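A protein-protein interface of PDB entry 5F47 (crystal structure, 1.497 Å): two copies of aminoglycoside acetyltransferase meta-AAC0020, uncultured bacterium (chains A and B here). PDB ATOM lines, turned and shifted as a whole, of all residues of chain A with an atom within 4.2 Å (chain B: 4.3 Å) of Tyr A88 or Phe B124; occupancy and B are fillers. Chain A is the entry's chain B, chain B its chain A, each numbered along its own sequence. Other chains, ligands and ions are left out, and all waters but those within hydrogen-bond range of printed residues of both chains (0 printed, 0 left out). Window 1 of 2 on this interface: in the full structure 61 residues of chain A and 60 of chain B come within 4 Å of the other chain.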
ATOM      1  N   THR A  73       5.032  35.050  28.306  1.00  0.00           N
ATOM      2  CA  THR A  73       5.518  34.900  26.941  1.00  0.00           C
ATOM      3  C   THR A  73       4.365  35.198  26.005  1.00  0.00           C
ATOM      4  O   THR A  73       3.206  34.912  26.336  1.00  0.00           O
ATOM      5  CB  THR A  73       6.041  33.484  26.690  1.00  0.00           C
ATOM      6  OG1 THR A  73       5.008  32.543  27.037  1.00  0.00           O
ATOM      7  CG2 THR A  73       7.269  33.211  27.554  1.00  0.00           C
ATOM      8  N   SER A  74       4.675  35.770  24.842  1.00  0.00           N
ATOM      9  CA  SER A  74       3.606  36.130  23.908  1.00  0.00           C
ATOM     10  C   SER A  74       4.092  35.962  22.461  1.00  0.00           C
ATOM     11  O   SER A  74       5.266  36.174  22.155  1.00  0.00           O
ATOM     12  CB  SER A  74       3.090  37.564  24.188  1.00  0.00           C
ATOM     13  OG  SER A  74       4.101  38.529  23.961  1.00  0.00           O
ATOM     14  N   TYR A  75       3.169  35.525  21.604  1.00  0.00           N
ATOM     15  CA  TYR A  75       3.410  35.306  20.177  1.00  0.00           C
ATOM     16  C   TYR A  75       2.561  36.254  19.350  1.00  0.00           C
ATOM     17  O   TYR A  75       1.359  36.399  19.590  1.00  0.00           O
ATOM     18  CB  TYR A  75       3.051  33.869  19.778  1.00  0.00           C
ATOM     19  CG  TYR A  75       3.910  32.806  20.405  1.00  0.00           C
ATOM     20  CD1 TYR A  75       3.599  32.301  21.665  1.00  0.00           C
ATOM     21  CD2 TYR A  75       5.010  32.297  19.736  1.00  0.00           C
ATOM     22  CE1 TYR A  75       4.383  31.309  22.252  1.00  0.00           C
ATOM     23  CE2 TYR A  75       5.812  31.292  20.314  1.00  0.00           C
ATOM     24  CZ  TYR A  75       5.489  30.820  21.583  1.00  0.00           C
ATOM     25  OH  TYR A  75       6.245  29.821  22.161  1.00  0.00           O
ATOM     26  N   LEU A  77       0.563  36.907  16.121  1.00  0.00           N
ATOM     27  CA  LEU A  77      -0.122  36.211  15.036  1.00  0.00           C
ATOM     28  C   LEU A  77      -0.654  37.218  14.019  1.00  0.00           C
ATOM     29  O   LEU A  77      -1.676  37.878  14.256  1.00  0.00           O
ATOM     30  CB  LEU A  77      -1.270  35.363  15.588  1.00  0.00           C
ATOM     31  CG  LEU A  77      -0.944  34.386  16.728  1.00  0.00           C
ATOM     32  CD1 LEU A  77      -2.215  33.658  17.166  1.00  0.00           C
ATOM     33  CD2 LEU A  77       0.162  33.388  16.349  1.00  0.00           C
ATOM     34  N   ALA A  87      -1.994  39.357  19.440  1.00  0.00           N
ATOM     35  CA  ALA A  87      -0.983  38.779  20.307  1.00  0.00           C
ATOM     36  C   ALA A  87      -1.594  37.701  21.193  1.00  0.00           C
ATOM     37  O   ALA A  87      -2.652  37.895  21.809  1.00  0.00           O
ATOM     38  CB  ALA A  87      -0.335  39.855  21.151  1.00  0.00           C
ATOM     39  N   TYR A  88      -0.897  36.580  21.274  1.00  0.00           N
ATOM     40  CA  TYR A  88      -1.305  35.405  22.033  1.00  0.00           C
ATOM     41  C   TYR A  88      -0.404  35.271  23.240  1.00  0.00           C
ATOM     42  O   TYR A  88       0.764  34.936  23.085  1.00  0.00           O
ATOM     43  CB  TYR A  88      -1.164  34.165  21.134  1.00  0.00           C
ATOM     44  CG  TYR A  88      -1.599  32.851  21.698  1.00  0.00           C
ATOM     45  CD1 TYR A  88      -2.399  32.759  22.824  1.00  0.00           C
ATOM     46  CD2 TYR A  88      -1.206  31.675  21.074  1.00  0.00           C
ATOM     47  CE1 TYR A  88      -2.794  31.525  23.315  1.00  0.00           C
ATOM     48  CE2 TYR A  88      -1.606  30.445  21.551  1.00  0.00           C
ATOM     49  CZ  TYR A  88      -2.402  30.375  22.664  1.00  0.00           C
ATOM     50  OH  TYR A  88      -2.793  29.148  23.125  1.00  0.00           O
ATOM     51  N   ILE A  89      -0.919  35.541  24.432  1.00  0.00           N
ATOM     52  CA  ILE A  89      -0.155  35.257  25.650  1.00  0.00           C
ATOM     53  C   ILE A  89      -0.208  33.758  25.892  1.00  0.00           C
ATOM     54  O   ILE A  89      -1.294  33.193  26.049  1.00  0.00           O
ATOM     55  CB  ILE A  89      -0.720  36.007  26.865  1.00  0.00           C
ATOM     56  CG1 ILE A  89      -0.586  37.521  26.661  1.00  0.00           C
ATOM     57  CG2 ILE A  89       0.022  35.578  28.146  1.00  0.00           C
ATOM     58  CD1 ILE A  89      -1.325  38.342  27.753  1.00  0.00           C
ATOM     59  N   TYR A  90       0.957  33.110  25.906  1.00  0.00           N
ATOM     60  CA  TYR A  90       0.975  31.671  26.008  1.00  0.00           C
ATOM     61  C   TYR A  90       1.109  31.179  27.451  1.00  0.00           C
ATOM     62  O   TYR A  90       0.384  30.269  27.871  1.00  0.00           O
ATOM     63  CB  TYR A  90       2.110  31.091  25.133  1.00  0.00           C
ATOM     64  CG  TYR A  90       2.002  29.597  25.038  1.00  0.00           C
ATOM     65  CD1 TYR A  90       1.119  28.999  24.138  1.00  0.00           C
ATOM     66  CD2 TYR A  90       2.723  28.780  25.906  1.00  0.00           C
ATOM     67  CE1 TYR A  90       0.994  27.598  24.087  1.00  0.00           C
ATOM     68  CE2 TYR A  90       2.600  27.391  25.864  1.00  0.00           C
ATOM     69  CZ  TYR A  90       1.741  26.810  24.957  1.00  0.00           C
ATOM     70  OH  TYR A  90       1.648  25.432  24.960  1.00  0.00           O
ATOM     71  N   PHE A 124      -4.957  37.998  23.422  1.00  0.00           N
ATOM     72  CA  PHE A 124      -5.760  36.967  24.083  1.00  0.00           C
ATOM     73  C   PHE A 124      -4.914  35.965  24.859  1.00  0.00           C
ATOM     74  O   PHE A 124      -3.700  35.852  24.659  1.00  0.00           O
ATOM     75  CB  PHE A 124      -6.686  36.242  23.073  1.00  0.00           C
ATOM     76  CG  PHE A 124      -5.965  35.442  22.003  1.00  0.00           C
ATOM     77  CD1 PHE A 124      -5.466  36.054  20.868  1.00  0.00           C
ATOM     78  CD2 PHE A 124      -5.824  34.077  22.134  1.00  0.00           C
ATOM     79  CE1 PHE A 124      -4.821  35.305  19.870  1.00  0.00           C
ATOM     80  CE2 PHE A 124      -5.207  33.328  21.137  1.00  0.00           C
ATOM     81  CZ  PHE A 124      -4.706  33.941  20.019  1.00  0.00           C
ATOM     82  N   GLN A 126      -5.421  32.122  27.522  1.00  0.00           N
ATOM     83  CA  GLN A 126      -6.309  31.068  27.982  1.00  0.00           C
ATOM     84  C   GLN A 126      -5.903  30.545  29.350  1.00  0.00           C
ATOM     85  O   GLN A 126      -4.745  30.656  29.766  1.00  0.00           O
ATOM     86  CB  GLN A 126      -6.339  29.945  26.953  1.00  0.00           C
ATOM     87  CG  GLN A 126      -7.012  30.360  25.655  1.00  0.00           C
ATOM     88  CD  GLN A 126      -6.173  30.074  24.450  1.00  0.00           C
ATOM     89  OE1 GLN A 126      -5.122  29.440  24.556  1.00  0.00           O
ATOM     90  NE2 GLN A 126      -6.616  30.544  23.292  1.00  0.00           N
ATOM     91  N   PHE A 152      -8.438  20.801  21.842  1.00  0.00           N
ATOM     92  CA  PHE A 152      -8.130  19.439  21.418  1.00  0.00           C
ATOM     93  C   PHE A 152      -6.665  19.377  21.045  1.00  0.00           C
ATOM     94  O   PHE A 152      -6.161  20.275  20.379  1.00  0.00           O
ATOM     95  CB  PHE A 152      -8.992  19.017  20.231  1.00  0.00           C
ATOM     96  CG  PHE A 152     -10.448  18.933  20.552  1.00  0.00           C
ATOM     97  CD1 PHE A 152     -11.274  20.025  20.354  1.00  0.00           C
ATOM     98  CD2 PHE A 152     -11.005  17.759  21.041  1.00  0.00           C
ATOM     99  CE1 PHE A 152     -12.635  19.956  20.657  1.00  0.00           C
ATOM    100  CE2 PHE A 152     -12.362  17.696  21.353  1.00  0.00           C
ATOM    101  CZ  PHE A 152     -13.172  18.785  21.143  1.00  0.00           C
ATOM    102  N   TYR A 153      -5.998  18.330  21.502  1.00  0.00           N
ATOM    103  CA  TYR A 153      -4.553  18.172  21.336  1.00  0.00           C
ATOM    104  C   TYR A 153      -4.241  16.903  20.576  1.00  0.00           C
ATOM    105  O   TYR A 153      -4.778  15.845  20.910  1.00  0.00           O
ATOM    106  CB  TYR A 153      -3.848  18.115  22.709  1.00  0.00           C
ATOM    107  CG  TYR A 153      -4.071  19.354  23.532  1.00  0.00           C
ATOM    108  CD1 TYR A 153      -3.265  20.472  23.353  1.00  0.00           C
ATOM    109  CD2 TYR A 153      -5.066  19.404  24.491  1.00  0.00           C
ATOM    110  CE1 TYR A 153      -3.459  21.620  24.098  1.00  0.00           C
ATOM    111  CE2 TYR A 153      -5.268  20.556  25.239  1.00  0.00           C
ATOM    112  CZ  TYR A 153      -4.459  21.640  25.038  1.00  0.00           C
ATOM    113  OH  TYR A 153      -4.665  22.782  25.792  1.00  0.00           O
ATOM    114  N   LEU B  77       4.283  27.675  16.506  1.00  0.00           N
ATOM    115  CA  LEU B  77       4.764  28.321  17.737  1.00  0.00           C
ATOM    116  C   LEU B  77       6.032  27.568  18.159  1.00  0.00           C
ATOM    117  O   LEU B  77       5.963  26.445  18.684  1.00  0.00           O
ATOM    118  CB  LEU B  77       3.707  28.267  18.838  1.00  0.00           C
ATOM    119  CG  LEU B  77       2.280  28.733  18.499  1.00  0.00           C
ATOM    120  CD1 LEU B  77       1.341  28.491  19.674  1.00  0.00           C
ATOM    121  CD2 LEU B  77       2.228  30.204  18.105  1.00  0.00           C
ATOM    122  N   ALA B  87       2.084  23.328  16.604  1.00  0.00           N
ATOM    123  CA  ALA B  87       1.241  23.983  15.603  1.00  0.00           C
ATOM    124  C   ALA B  87      -0.128  24.288  16.182  1.00  0.00           C
ATOM    125  O   ALA B  87      -0.740  23.453  16.846  1.00  0.00           O
ATOM    126  CB  ALA B  87       1.092  23.126  14.368  1.00  0.00           C
ATOM    127  N   TYR B  88      -0.593  25.500  15.913  1.00  0.00           N
ATOM    128  CA  TYR B  88      -1.875  26.004  16.384  1.00  0.00           C
ATOM    129  C   TYR B  88      -2.803  26.131  15.183  1.00  0.00           C
ATOM    130  O   TYR B  88      -2.611  27.012  14.336  1.00  0.00           O
ATOM    131  CB  TYR B  88      -1.652  27.363  17.060  1.00  0.00           C
ATOM    132  CG  TYR B  88      -2.843  28.120  17.623  1.00  0.00           C
ATOM    133  CD1 TYR B  88      -4.069  27.524  17.839  1.00  0.00           C
ATOM    134  CD2 TYR B  88      -2.703  29.461  17.946  1.00  0.00           C
ATOM    135  CE1 TYR B  88      -5.145  28.251  18.363  1.00  0.00           C
ATOM    136  CE2 TYR B  88      -3.747  30.191  18.468  1.00  0.00           C
ATOM    137  CZ  TYR B  88      -4.959  29.585  18.671  1.00  0.00           C
ATOM    138  OH  TYR B  88      -5.989  30.335  19.194  1.00  0.00           O
ATOM    139  N   ILE B  89      -3.766  25.226  15.083  1.00  0.00           N
ATOM    140  CA  ILE B  89      -4.810  25.343  14.059  1.00  0.00           C
ATOM    141  C   ILE B  89      -5.737  26.479  14.462  1.00  0.00           C
ATOM    142  O   ILE B  89      -6.330  26.455  15.553  1.00  0.00           O
ATOM    143  CB  ILE B  89      -5.602  24.043  13.911  1.00  0.00           C
ATOM    144  CG1 ILE B  89      -4.692  22.897  13.416  1.00  0.00           C
ATOM    145  CG2 ILE B  89      -6.785  24.302  12.954  1.00  0.00           C
ATOM    146  CD1 ILE B  89      -5.369  21.534  13.498  1.00  0.00           C
ATOM    147  N   VAL B 123      -0.064  19.377  17.919  1.00  0.00           N
ATOM    148  CA  VAL B 123      -0.941  20.282  17.184  1.00  0.00           C
ATOM    149  C   VAL B 123      -2.153  20.500  18.074  1.00  0.00           C
ATOM    150  O   VAL B 123      -2.611  19.578  18.732  1.00  0.00           O
ATOM    151  CB  VAL B 123      -1.376  19.686  15.833  1.00  0.00           C
ATOM    152  CG1 VAL B 123      -2.284  20.619  15.063  1.00  0.00           C
ATOM    153  CG2 VAL B 123      -0.152  19.331  14.957  1.00  0.00           C
ATOM    154  N   PHE B 124      -2.684  21.718  18.131  1.00  0.00           N
ATOM    155  CA  PHE B 124      -3.894  21.903  18.925  1.00  0.00           C
ATOM    156  C   PHE B 124      -4.838  22.859  18.249  1.00  0.00           C
ATOM    157  O   PHE B 124      -4.452  23.614  17.354  1.00  0.00           O
ATOM    158  CB  PHE B 124      -3.569  22.375  20.363  1.00  0.00           C
ATOM    159  CG  PHE B 124      -3.017  23.786  20.464  1.00  0.00           C
ATOM    160  CD1 PHE B 124      -1.696  24.062  20.138  1.00  0.00           C
ATOM    161  CD2 PHE B 124      -3.815  24.811  20.912  1.00  0.00           C
ATOM    162  CE1 PHE B 124      -1.186  25.364  20.251  1.00  0.00           C
ATOM    163  CE2 PHE B 124      -3.314  26.127  21.026  1.00  0.00           C
ATOM    164  CZ  PHE B 124      -2.004  26.388  20.702  1.00  0.00           C
ATOM    165  N   VAL B 125      -6.077  22.831  18.714  1.00  0.00           N
ATOM    166  CA  VAL B 125      -7.154  23.604  18.092  1.00  0.00           C
ATOM    167  C   VAL B 125      -8.208  23.921  19.149  1.00  0.00           C
ATOM    168  O   VAL B 125      -8.400  23.187  20.113  1.00  0.00           O
ATOM    169  CB  VAL B 125      -7.762  22.824  16.895  1.00  0.00           C
ATOM    170  CG1 VAL B 125      -8.438  21.553  17.359  1.00  0.00           C
ATOM    171  CG2 VAL B 125      -8.774  23.690  16.126  1.00  0.00           C
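The backbone carbonyl oxygen of Val B125 is in hydrogen-bond range of the backbone NH of Phe A152 (2.9 Å).
N of Ile A89 lies within hydrogen-bond range of O of Phe A124.
The side-chain hydroxyl (OH) of Tyr A88 is in hydrogen-bond range of the side-chain amide oxygen (OE1) of Gln A126 (2.7 Å).
The backbone NH (N) of Phe A124 sits at hydrogen-bond distance from the backbone carbonyl oxygen (O) of Ala A87 (2.8 Å).
The backbone carbonyl oxygen (O) of Ala B87 is in hydrogen-bond range of the backbone NH (N) of Phe B124 (2.9 Å).
N of Tyr A88 sits at hydrogen-bond distance from O of Tyr A75.
The backbone NH (N) of Ile B89 is in hydrogen-bond range of the backbone carbonyl oxygen (O) of Phe B124, at 2.9 Å.
CD2 of Tyr A75 touches CD2 of Leu B77, at 3.8 Å.
CE2 of Tyr B88 touches CE2 of Tyr A88, 3.8 Å away.
CE2 of Phe B124 touches OH of Tyr A88 (3.7 Å).
CE2 of Phe A124 touches OH of Tyr B88 (3.7 Å).
O of Val B123 touches O of Phe A152, at 3.98 Å.
Phe B124 touches Phe A152.
Tyr A153 touches Val B123 (CA to O, 3.5 Å).
Phe B124 touches Tyr A153 (CB to CD1, 3.6 Å).
Printed residues of chain B within 4 Å of Tyr A88: Tyr B88 and Phe B124.
Of the printed residues of chain B, Phe A152 touches Val B123 (3.98 Å), Phe B124 (3.1 Å) and Val B125 (2.9 Å).
Printed residues of chain B within 4 Å of Tyr A153: Val B123 (3.5 Å) and Phe B124 (3.6 Å).
Of the printed residues of chain A, Val B123 touches Phe A152 (3.98 Å) and Tyr A153 (3.5 Å).
Phe B124 touches three residues of chain A.
Printed residues of chain A within 4 Å of Val B125: Phe A152 (2.9 Å).
The nearest printed residue of chain B that does not touch Tyr A88 is Leu B77 (4.003 Å).
The nearest printed residue of chain A that does not touch Phe B124 is Tyr A90 (4.7 Å).
The nearest printed residue of chain A that does not touch Tyr B88 is Leu A77 (4.01 Å).
Of the 12 printed residues of chain A, 5 touch a printed residue of chain B.
Of the 7 printed residues of chain B, 5 touch a printed residue of chain A.
Printed residues of chain B that touch a printed residue of chain A: Leu B77, Tyr B88, Val B123, Phe B124 and Val B125.
Hydrophobic or aromatic side chains of chain B within 4 Å of the printed part of chain A: Leu B77, Tyr B88, Phe B124 and Val B125.
Among the printed residues, 9 pairs touch across the chains.
Among the printed residues, no Asp or Glu carboxylate lies within 4 Å of a Lys or Arg side-chain nitrogen of the other chain.
Tyr A88 touches its own counterpart, Tyr B88.
Tyr A88 touches Phe B124, and with the chains exchanged Phe A124 touches Tyr B88.
Positions printed for both chains: 77, 87, 88, 89 and 124.
Of the 9 pairs that touch across the chains among the printed residues, 3 have their exchanged pair printed and touching as well.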
